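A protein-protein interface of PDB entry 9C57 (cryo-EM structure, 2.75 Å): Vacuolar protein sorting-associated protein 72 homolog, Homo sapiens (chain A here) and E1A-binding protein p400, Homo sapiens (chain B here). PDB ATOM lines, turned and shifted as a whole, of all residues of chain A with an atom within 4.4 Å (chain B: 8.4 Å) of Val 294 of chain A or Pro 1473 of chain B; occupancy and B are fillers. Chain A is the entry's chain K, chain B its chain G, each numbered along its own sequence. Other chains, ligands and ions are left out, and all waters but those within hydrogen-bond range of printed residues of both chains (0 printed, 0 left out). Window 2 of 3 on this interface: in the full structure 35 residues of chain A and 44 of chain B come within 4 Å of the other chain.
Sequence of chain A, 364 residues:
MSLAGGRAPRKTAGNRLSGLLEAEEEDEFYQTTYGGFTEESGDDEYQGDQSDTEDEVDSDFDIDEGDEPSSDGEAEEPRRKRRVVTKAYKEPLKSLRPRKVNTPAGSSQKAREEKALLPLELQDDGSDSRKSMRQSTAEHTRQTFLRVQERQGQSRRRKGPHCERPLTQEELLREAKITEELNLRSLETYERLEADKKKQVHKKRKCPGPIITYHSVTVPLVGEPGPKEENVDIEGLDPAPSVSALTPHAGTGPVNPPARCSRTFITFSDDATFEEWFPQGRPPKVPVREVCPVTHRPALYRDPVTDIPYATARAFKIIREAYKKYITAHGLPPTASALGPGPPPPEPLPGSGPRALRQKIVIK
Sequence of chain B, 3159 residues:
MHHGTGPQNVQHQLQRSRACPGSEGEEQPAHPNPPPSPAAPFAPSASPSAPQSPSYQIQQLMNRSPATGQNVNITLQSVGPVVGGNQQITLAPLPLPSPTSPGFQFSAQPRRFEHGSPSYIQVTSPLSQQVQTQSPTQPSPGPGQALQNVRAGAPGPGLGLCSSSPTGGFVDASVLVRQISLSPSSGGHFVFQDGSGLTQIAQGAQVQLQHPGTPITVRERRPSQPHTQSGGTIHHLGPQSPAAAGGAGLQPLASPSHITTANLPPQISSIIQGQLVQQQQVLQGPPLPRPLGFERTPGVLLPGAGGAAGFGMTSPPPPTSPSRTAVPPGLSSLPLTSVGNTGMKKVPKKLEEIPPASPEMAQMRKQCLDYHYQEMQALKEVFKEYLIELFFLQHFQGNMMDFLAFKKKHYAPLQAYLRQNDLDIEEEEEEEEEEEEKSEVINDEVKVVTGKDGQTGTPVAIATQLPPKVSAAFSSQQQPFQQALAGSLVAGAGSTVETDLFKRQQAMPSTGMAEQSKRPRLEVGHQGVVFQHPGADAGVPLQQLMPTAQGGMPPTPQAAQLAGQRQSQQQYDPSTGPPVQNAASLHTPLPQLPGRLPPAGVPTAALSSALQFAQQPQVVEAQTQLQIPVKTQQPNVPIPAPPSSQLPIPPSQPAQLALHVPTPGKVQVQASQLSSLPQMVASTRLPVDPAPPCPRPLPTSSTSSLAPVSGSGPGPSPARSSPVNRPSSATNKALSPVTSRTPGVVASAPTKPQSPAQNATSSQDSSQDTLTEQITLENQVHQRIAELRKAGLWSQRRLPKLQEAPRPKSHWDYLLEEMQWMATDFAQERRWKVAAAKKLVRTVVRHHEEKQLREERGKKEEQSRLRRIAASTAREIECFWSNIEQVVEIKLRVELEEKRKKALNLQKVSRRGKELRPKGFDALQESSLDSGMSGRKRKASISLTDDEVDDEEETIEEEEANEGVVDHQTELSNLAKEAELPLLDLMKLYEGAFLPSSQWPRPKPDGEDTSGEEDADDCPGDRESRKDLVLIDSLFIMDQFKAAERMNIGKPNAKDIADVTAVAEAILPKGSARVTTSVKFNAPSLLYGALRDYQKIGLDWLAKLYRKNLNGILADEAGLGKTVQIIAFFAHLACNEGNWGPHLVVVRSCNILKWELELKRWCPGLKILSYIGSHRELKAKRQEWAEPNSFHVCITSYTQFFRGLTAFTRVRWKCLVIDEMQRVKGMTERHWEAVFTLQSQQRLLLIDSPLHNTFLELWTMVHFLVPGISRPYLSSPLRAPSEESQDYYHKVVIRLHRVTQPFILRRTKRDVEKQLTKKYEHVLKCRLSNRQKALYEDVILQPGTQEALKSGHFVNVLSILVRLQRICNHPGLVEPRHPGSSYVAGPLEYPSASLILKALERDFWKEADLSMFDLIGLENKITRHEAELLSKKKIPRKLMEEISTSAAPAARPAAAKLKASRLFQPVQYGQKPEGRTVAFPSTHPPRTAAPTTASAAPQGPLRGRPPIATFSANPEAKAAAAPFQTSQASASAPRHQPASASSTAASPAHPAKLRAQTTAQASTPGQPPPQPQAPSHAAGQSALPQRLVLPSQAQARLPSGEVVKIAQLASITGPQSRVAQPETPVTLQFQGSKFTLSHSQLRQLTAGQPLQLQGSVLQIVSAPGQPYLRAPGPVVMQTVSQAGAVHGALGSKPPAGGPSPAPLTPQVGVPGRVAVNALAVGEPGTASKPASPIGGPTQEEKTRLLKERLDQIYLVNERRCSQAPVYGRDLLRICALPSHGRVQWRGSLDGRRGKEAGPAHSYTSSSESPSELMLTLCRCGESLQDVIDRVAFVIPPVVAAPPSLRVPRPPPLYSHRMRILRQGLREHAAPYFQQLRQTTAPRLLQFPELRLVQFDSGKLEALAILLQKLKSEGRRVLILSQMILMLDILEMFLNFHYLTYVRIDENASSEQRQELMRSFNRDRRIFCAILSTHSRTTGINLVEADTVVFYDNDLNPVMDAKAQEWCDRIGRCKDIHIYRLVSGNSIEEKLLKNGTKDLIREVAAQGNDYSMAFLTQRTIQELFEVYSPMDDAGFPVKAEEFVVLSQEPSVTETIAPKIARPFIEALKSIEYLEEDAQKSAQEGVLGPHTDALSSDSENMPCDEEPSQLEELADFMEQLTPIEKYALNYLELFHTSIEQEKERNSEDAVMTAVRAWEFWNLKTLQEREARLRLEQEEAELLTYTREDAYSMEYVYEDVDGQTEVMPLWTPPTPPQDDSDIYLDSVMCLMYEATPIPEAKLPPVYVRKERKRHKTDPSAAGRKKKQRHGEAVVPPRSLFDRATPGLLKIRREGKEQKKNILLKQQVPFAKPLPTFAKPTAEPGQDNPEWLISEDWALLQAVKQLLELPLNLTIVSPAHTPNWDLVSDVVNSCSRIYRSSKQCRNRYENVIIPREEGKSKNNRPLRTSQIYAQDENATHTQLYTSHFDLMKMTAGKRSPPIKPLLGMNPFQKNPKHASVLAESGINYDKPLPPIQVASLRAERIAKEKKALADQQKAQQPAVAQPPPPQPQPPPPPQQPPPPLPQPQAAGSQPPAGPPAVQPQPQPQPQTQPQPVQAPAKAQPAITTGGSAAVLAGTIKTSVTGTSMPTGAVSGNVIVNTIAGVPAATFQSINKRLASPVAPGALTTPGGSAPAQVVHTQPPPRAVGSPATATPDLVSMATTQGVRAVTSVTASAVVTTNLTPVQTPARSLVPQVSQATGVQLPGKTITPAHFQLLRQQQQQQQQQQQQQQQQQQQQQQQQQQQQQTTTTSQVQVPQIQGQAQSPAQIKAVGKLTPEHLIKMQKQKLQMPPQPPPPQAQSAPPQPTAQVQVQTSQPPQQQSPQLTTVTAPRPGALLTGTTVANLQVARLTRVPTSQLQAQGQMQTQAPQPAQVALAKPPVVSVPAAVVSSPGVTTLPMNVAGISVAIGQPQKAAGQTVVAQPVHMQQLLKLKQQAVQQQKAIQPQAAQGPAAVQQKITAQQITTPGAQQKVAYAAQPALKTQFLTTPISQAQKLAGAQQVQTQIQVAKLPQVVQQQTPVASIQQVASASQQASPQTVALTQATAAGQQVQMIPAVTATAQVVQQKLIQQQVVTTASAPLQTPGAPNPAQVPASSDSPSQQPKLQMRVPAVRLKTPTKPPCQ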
ATOM      1  N   CYS A 292     -15.060 -16.794  26.400  1.00  0.00           N
ATOM      2  CA  CYS A 292     -14.627 -18.183  26.490  1.00  0.00           C
ATOM      3  C   CYS A 292     -14.034 -18.623  25.156  1.00  0.00           C
ATOM      4  O   CYS A 292     -14.728 -18.565  24.136  1.00  0.00           O
ATOM      5  CB  CYS A 292     -15.794 -19.086  26.863  1.00  0.00           C
ATOM      6  SG  CYS A 292     -15.426 -20.847  26.741  1.00  0.00           S
ATOM      7  N   PRO A 293     -12.778 -19.070  25.112  1.00  0.00           N
ATOM      8  CA  PRO A 293     -12.190 -19.432  23.813  1.00  0.00           C
ATOM      9  C   PRO A 293     -12.956 -20.510  23.069  1.00  0.00           C
ATOM     10  O   PRO A 293     -12.987 -20.488  21.833  1.00  0.00           O
ATOM     11  CB  PRO A 293     -10.780 -19.902  24.189  1.00  0.00           C
ATOM     12  CG  PRO A 293     -10.492 -19.245  25.479  1.00  0.00           C
ATOM     13  CD  PRO A 293     -11.794 -19.176  26.202  1.00  0.00           C
ATOM     14  N   VAL A 294     -13.575 -21.454  23.772  1.00  0.00           N
ATOM     15  CA  VAL A 294     -14.242 -22.565  23.100  1.00  0.00           C
ATOM     16  C   VAL A 294     -15.567 -22.116  22.497  1.00  0.00           C
ATOM     17  O   VAL A 294     -15.774 -22.194  21.281  1.00  0.00           O
ATOM     18  CB  VAL A 294     -14.443 -23.741  24.071  1.00  0.00           C
ATOM     19  CG1 VAL A 294     -15.343 -24.790  23.446  1.00  0.00           C
ATOM     20  CG2 VAL A 294     -13.107 -24.344  24.450  1.00  0.00           C
ATOM     21  N   THR A 295     -16.483 -21.644  23.336  1.00  0.00           N
ATOM     22  CA  THR A 295     -17.818 -21.271  22.890  1.00  0.00           C
ATOM     23  C   THR A 295     -17.954 -19.787  22.568  1.00  0.00           C
ATOM     24  O   THR A 295     -19.021 -19.367  22.113  1.00  0.00           O
ATOM     25  CB  THR A 295     -18.862 -21.664  23.944  1.00  0.00           C
ATOM     26  OG1 THR A 295     -20.136 -21.114  23.589  1.00  0.00           O
ATOM     27  CG2 THR A 295     -18.464 -21.170  25.323  1.00  0.00           C
ATOM     28  N   HIS A 296     -16.906 -18.991  22.779  1.00  0.00           N
ATOM     29  CA  HIS A 296     -16.954 -17.549  22.521  1.00  0.00           C
ATOM     30  C   HIS A 296     -18.145 -16.902  23.217  1.00  0.00           C
ATOM     31  O   HIS A 296     -18.681 -15.888  22.766  1.00  0.00           O
ATOM     32  CB  HIS A 296     -16.969 -17.257  21.021  1.00  0.00           C
ATOM     33  CG  HIS A 296     -15.657 -17.512  20.350  1.00  0.00           C
ATOM     34  ND1 HIS A 296     -15.375 -17.083  19.073  1.00  0.00           N
ATOM     35  CD2 HIS A 296     -14.548 -18.153  20.786  1.00  0.00           C
ATOM     36  CE1 HIS A 296     -14.147 -17.447  18.751  1.00  0.00           C
ATOM     37  NE2 HIS A 296     -13.624 -18.099  19.772  1.00  0.00           N
ATOM     38  N   ARG A 314     -17.809 -28.264  29.380  1.00  0.00           N
ATOM     39  CA  ARG A 314     -17.178 -28.762  28.165  1.00  0.00           C
ATOM     40  C   ARG A 314     -15.973 -27.911  27.808  1.00  0.00           C
ATOM     41  O   ARG A 314     -14.906 -28.433  27.462  1.00  0.00           O
ATOM     42  CB  ARG A 314     -18.178 -28.770  27.012  1.00  0.00           C
ATOM     43  CG  ARG A 314     -17.580 -29.246  25.702  1.00  0.00           C
ATOM     44  CD  ARG A 314     -18.627 -29.389  24.617  1.00  0.00           C
ATOM     45  NE  ARG A 314     -18.837 -28.141  23.893  1.00  0.00           N
ATOM     46  CZ  ARG A 314     -18.218 -27.808  22.768  1.00  0.00           C
ATOM     47  NH1 ARG A 314     -17.308 -28.594  22.218  1.00  0.00           N
ATOM     48  NH2 ARG A 314     -18.517 -26.654  22.181  1.00  0.00           N
ATOM     49  N   ALA A 315     -16.129 -26.590  27.893  1.00  0.00           N
ATOM     50  CA  ALA A 315     -15.005 -25.697  27.660  1.00  0.00           C
ATOM     51  C   ALA A 315     -13.876 -25.987  28.635  1.00  0.00           C
ATOM     52  O   ALA A 315     -12.701 -25.925  28.266  1.00  0.00           O
ATOM     53  CB  ALA A 315     -15.456 -24.244  27.778  1.00  0.00           C
ATOM     54  N   ILE A 318     -12.059 -29.187  27.555  1.00  0.00           N
ATOM     55  CA  ILE A 318     -11.324 -28.914  26.323  1.00  0.00           C
ATOM     56  C   ILE A 318     -10.082 -28.082  26.618  1.00  0.00           C
ATOM     57  O   ILE A 318      -8.998 -28.344  26.083  1.00  0.00           O
ATOM     58  CB  ILE A 318     -12.241 -28.229  25.295  1.00  0.00           C
ATOM     59  CG1 ILE A 318     -13.302 -29.216  24.807  1.00  0.00           C
ATOM     60  CG2 ILE A 318     -11.425 -27.703  24.126  1.00  0.00           C
ATOM     61  CD1 ILE A 318     -14.361 -28.604  23.928  1.00  0.00           C
ATOM     62  N   ALA B1460      -5.147 -16.951  26.187  1.00  0.00           N
ATOM     63  CA  ALA B1460      -6.180 -17.696  25.478  1.00  0.00           C
ATOM     64  C   ALA B1460      -5.725 -18.085  24.077  1.00  0.00           C
ATOM     65  O   ALA B1460      -5.980 -19.206  23.622  1.00  0.00           O
ATOM     66  CB  ALA B1460      -7.466 -16.875  25.410  1.00  0.00           C
ATOM     67  N   PHE B1464      -5.564 -22.751  21.571  1.00  0.00           N
ATOM     68  CA  PHE B1464      -6.729 -22.394  20.772  1.00  0.00           C
ATOM     69  C   PHE B1464      -6.337 -21.585  19.543  1.00  0.00           C
ATOM     70  O   PHE B1464      -5.149 -21.409  19.261  1.00  0.00           O
ATOM     71  CB  PHE B1464      -7.732 -21.616  21.624  1.00  0.00           C
ATOM     72  CG  PHE B1464      -8.365 -22.439  22.695  1.00  0.00           C
ATOM     73  CD1 PHE B1464      -9.363 -23.344  22.385  1.00  0.00           C
ATOM     74  CD2 PHE B1464      -7.952 -22.326  24.006  1.00  0.00           C
ATOM     75  CE1 PHE B1464      -9.943 -24.109  23.362  1.00  0.00           C
ATOM     76  CE2 PHE B1464      -8.528 -23.091  24.988  1.00  0.00           C
ATOM     77  CZ  PHE B1464      -9.526 -23.984  24.666  1.00  0.00           C
ATOM     78  N   GLN B1465      -7.325 -21.088  18.810  1.00  0.00           N
ATOM     79  CA  GLN B1465      -7.069 -20.421  17.543  1.00  0.00           C
ATOM     80  C   GLN B1465      -8.266 -19.553  17.176  1.00  0.00           C
ATOM     81  O   GLN B1465      -9.409 -20.016  17.269  1.00  0.00           O
ATOM     82  CB  GLN B1465      -6.796 -21.461  16.458  1.00  0.00           C
ATOM     83  CG  GLN B1465      -5.903 -20.990  15.340  1.00  0.00           C
ATOM     84  CD  GLN B1465      -5.636 -22.084  14.335  1.00  0.00           C
ATOM     85  OE1 GLN B1465      -4.574 -22.703  14.341  1.00  0.00           O
ATOM     86  NE2 GLN B1465      -6.608 -22.342  13.470  1.00  0.00           N
ATOM     87  N   PRO B1466      -8.062 -18.303  16.758  1.00  0.00           N
ATOM     88  CA  PRO B1466      -9.210 -17.421  16.519  1.00  0.00           C
ATOM     89  C   PRO B1466     -10.154 -17.986  15.470  1.00  0.00           C
ATOM     90  O   PRO B1466      -9.749 -18.713  14.560  1.00  0.00           O
ATOM     91  CB  PRO B1466      -8.562 -16.115  16.046  1.00  0.00           C
ATOM     92  CG  PRO B1466      -7.200 -16.147  16.609  1.00  0.00           C
ATOM     93  CD  PRO B1466      -6.787 -17.585  16.593  1.00  0.00           C
ATOM     94  N   VAL B1467     -11.430 -17.648  15.617  1.00  0.00           N
ATOM     95  CA  VAL B1467     -12.488 -18.138  14.744  1.00  0.00           C
ATOM     96  C   VAL B1467     -12.895 -17.025  13.791  1.00  0.00           C
ATOM     97  O   VAL B1467     -13.109 -15.881  14.209  1.00  0.00           O
ATOM     98  CB  VAL B1467     -13.698 -18.628  15.555  1.00  0.00           C
ATOM     99  CG1 VAL B1467     -14.773 -19.161  14.629  1.00  0.00           C
ATOM    100  CG2 VAL B1467     -13.272 -19.691  16.550  1.00  0.00           C
ATOM    101  N   GLN B1468     -12.999 -17.360  12.512  1.00  0.00           N
ATOM    102  CA  GLN B1468     -13.475 -16.411  11.520  1.00  0.00           C
ATOM    103  C   GLN B1468     -14.922 -16.033  11.809  1.00  0.00           C
ATOM    104  O   GLN B1468     -15.745 -16.885  12.151  1.00  0.00           O
ATOM    105  CB  GLN B1468     -13.354 -17.024  10.128  1.00  0.00           C
ATOM    106  CG  GLN B1468     -13.603 -16.074   8.992  1.00  0.00           C
ATOM    107  CD  GLN B1468     -13.273 -16.699   7.660  1.00  0.00           C
ATOM    108  OE1 GLN B1468     -14.161 -16.997   6.864  1.00  0.00           O
ATOM    109  NE2 GLN B1468     -11.989 -16.921   7.416  1.00  0.00           N
ATOM    110  N   GLY B1470     -18.640 -15.528  11.793  1.00  0.00           N
ATOM    111  CA  GLY B1470     -19.661 -16.324  11.158  1.00  0.00           C
ATOM    112  C   GLY B1470     -19.481 -17.818  11.325  1.00  0.00           C
ATOM    113  O   GLY B1470     -20.469 -18.556  11.258  1.00  0.00           O
ATOM    114  N   GLN B1471     -18.253 -18.282  11.538  1.00  0.00           N
ATOM    115  CA  GLN B1471     -18.021 -19.682  11.851  1.00  0.00           C
ATOM    116  C   GLN B1471     -18.346 -19.937  13.314  1.00  0.00           C
ATOM    117  O   GLN B1471     -17.952 -19.162  14.191  1.00  0.00           O
ATOM    118  CB  GLN B1471     -16.575 -20.069  11.557  1.00  0.00           C
ATOM    119  CG  GLN B1471     -16.258 -20.196  10.088  1.00  0.00           C
ATOM    120  CD  GLN B1471     -14.867 -20.734   9.853  1.00  0.00           C
ATOM    121  OE1 GLN B1471     -14.100 -20.930  10.793  1.00  0.00           O
ATOM    122  NE2 GLN B1471     -14.530 -20.975   8.593  1.00  0.00           N
ATOM    123  N   LYS B1472     -19.067 -21.016  13.576  1.00  0.00           N
ATOM    124  CA  LYS B1472     -19.458 -21.321  14.941  1.00  0.00           C
ATOM    125  C   LYS B1472     -18.216 -21.622  15.774  1.00  0.00           C
ATOM    126  O   LYS B1472     -17.303 -22.302  15.288  1.00  0.00           O
ATOM    127  CB  LYS B1472     -20.416 -22.510  14.971  1.00  0.00           C
ATOM    128  CG  LYS B1472     -21.715 -22.285  14.215  1.00  0.00           C
ATOM    129  CD  LYS B1472     -22.368 -20.960  14.584  1.00  0.00           C
ATOM    130  CE  LYS B1472     -23.888 -21.035  14.560  1.00  0.00           C
ATOM    131  NZ  LYS B1472     -24.433 -22.150  15.385  1.00  0.00           N
ATOM    132  N   PRO B1473     -18.136 -21.143  17.014  1.00  0.00           N
ATOM    133  CA  PRO B1473     -16.925 -21.385  17.806  1.00  0.00           C
ATOM    134  C   PRO B1473     -16.767 -22.859  18.146  1.00  0.00           C
ATOM    135  O   PRO B1473     -17.639 -23.469  18.767  1.00  0.00           O
ATOM    136  CB  PRO B1473     -17.146 -20.537  19.066  1.00  0.00           C
ATOM    137  CG  PRO B1473     -18.290 -19.643  18.760  1.00  0.00           C
ATOM    138  CD  PRO B1473     -19.122 -20.346  17.758  1.00  0.00           C
ATOM    139  N   GLU B1474     -15.641 -23.429  17.731  1.00  0.00           N
ATOM    140  CA  GLU B1474     -15.261 -24.772  18.129  1.00  0.00           C
ATOM    141  C   GLU B1474     -13.780 -24.765  18.464  1.00  0.00           C
ATOM    142  O   GLU B1474     -13.001 -24.000  17.890  1.00  0.00           O
ATOM    143  CB  GLU B1474     -15.559 -25.808  17.033  1.00  0.00           C
ATOM    144  CG  GLU B1474     -17.000 -26.340  16.967  1.00  0.00           C
ATOM    145  CD  GLU B1474     -17.721 -26.420  18.308  1.00  0.00           C
ATOM    146  OE1 GLU B1474     -18.968 -26.361  18.305  1.00  0.00           O
ATOM    147  OE2 GLU B1474     -17.064 -26.618  19.352  1.00  0.00           O
ATOM    148  N   GLY B1475     -13.399 -25.629  19.396  1.00  0.00           N
ATOM    149  CA  GLY B1475     -12.097 -25.532  20.019  1.00  0.00           C
ATOM    150  C   GLY B1475     -10.944 -25.911  19.117  1.00  0.00           C
ATOM    151  O   GLY B1475     -10.162 -26.806  19.449  1.00  0.00           O
ATOM    152  N   ARG B1476     -10.822 -25.242  17.976  1.00  0.00           N
ATOM    153  CA  ARG B1476      -9.635 -25.411  17.155  1.00  0.00           C
ATOM    154  C   ARG B1476      -8.412 -25.013  17.966  1.00  0.00           C
ATOM    155  O   ARG B1476      -8.382 -23.940  18.575  1.00  0.00           O
ATOM    156  CB  ARG B1476      -9.740 -24.564  15.889  1.00  0.00           C
ATOM    157  CG  ARG B1476      -8.707 -24.900  14.824  1.00  0.00           C
ATOM    158  CD  ARG B1476      -8.948 -26.266  14.200  1.00  0.00           C
ATOM    159  NE  ARG B1476     -10.344 -26.478  13.839  1.00  0.00           N
ATOM    160  CZ  ARG B1476     -10.977 -25.832  12.870  1.00  0.00           C
ATOM    161  NH1 ARG B1476     -10.365 -24.921  12.131  1.00  0.00           N
ATOM    162  NH2 ARG B1476     -12.256 -26.107  12.635  1.00  0.00           N
ATOM    163  N   THR B1477      -7.404 -25.876  17.974  1.00  0.00           N
ATOM    164  CA  THR B1477      -6.250 -25.711  18.842  1.00  0.00           C
ATOM    165  C   THR B1477      -4.976 -25.651  18.016  1.00  0.00           C
ATOM    166  O   THR B1477      -4.757 -26.486  17.134  1.00  0.00           O
ATOM    167  CB  THR B1477      -6.162 -26.855  19.852  1.00  0.00           C
ATOM    168  OG1 THR B1477      -6.513 -28.086  19.210  1.00  0.00           O
ATOM    169  CG2 THR B1477      -7.104 -26.607  21.014  1.00  0.00           C
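The guanidinium group (NH2) of Arg 314 of chain A lies within salt-bridge range of the side-chain carboxylate (OE2) of Glu 1474 of chain B (3.2 Å). The backbone carbonyl oxygen of Val 294 of chain A lies close to the backbone carbonyl oxygen of Pro 1473 of chain B (3.4 Å).
SG of Cys 292 of chain A lies close to N of Val 294 of chain A (3.6 Å). SG of Cys 292 of chain A lies close to N of Thr 295 of chain A (3.7 Å). The backbone carbonyl oxygen of Pro 293 of chain A lies close to a ring nitrogen (NE2) of His 296 of chain A, 3.2 Å away.
Among the printed residues, pairs that only touch across the chains: Pro 293 of chain A with Ala 1460 of chain B (3.8 Å), Pro 293 of chain A with Phe 1464 of chain B (3.7 Å), Val 294 of chain A with Phe 1464 of chain B (3.4 Å), Val 294 of chain A with Glu 1474 of chain B (3.8 Å), Thr 295 of chain A with Pro 1473 of chain B (3.4 Å), His 296 of chain A with Val 1467 of chain B (3.3 Å), His 296 of chain A with Pro 1473 of chain B (3.5 Å) and Ile 318 of chain A with Phe 1464 of chain B (3.96 Å).
Val 294 of chain A touches just these residues of chain B: Phe 1464, Pro 1473 and Glu 1474. Of the printed residues of chain A, Pro 1473 of chain B touches Val 294 (3.1 Å), Thr 295 (3.4 Å) and His 296 (3.5 Å). Printed residues of chain A within 4 Å of Ala 1460 of chain B: Pro 293 (3.8 Å). Of the printed residues of chain A, Glu 1474 of chain B touches Val 294 (3.8 Å) and Arg 314 (3.2 Å). Printed residues of chain B within 4 Å of Ile 318 of chain A: Phe 1464. Of the printed residues of chain A, Phe 1464 of chain B touches Pro 293 (3.7 Å), Val 294 (3.4 Å) and Ile 318 (3.96 Å). The nearest residue of chain B that does not touch Val 294 of chain A is Gly 1475 of chain B (4.6 Å).
Of the 8 printed residues of chain A, 6 touch a printed residue of chain B. Printed residues of chain A that touch a printed residue of chain B: Pro 293, Val 294, Thr 295, His 296, Arg 314 and Ile 318. Hydrophobic or aromatic side chains of chain A that line the printed part of chain B: Pro 293, Val 294, His 296 and Ile 318. Of the 14 printed residues of chain B, 5 touch a printed residue of chain A. Hydrophobic or aromatic side chains of chain B that line the printed part of chain A: Ala 1460, Phe 1464, Val 1467 and Pro 1473. Among the printed residues, Asp or Glu carboxylates within 4 Å of a Lys or Arg side-chain nitrogen of the other chain: Arg 314 of chain A with Glu 1474 of chain B (3.2 Å).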
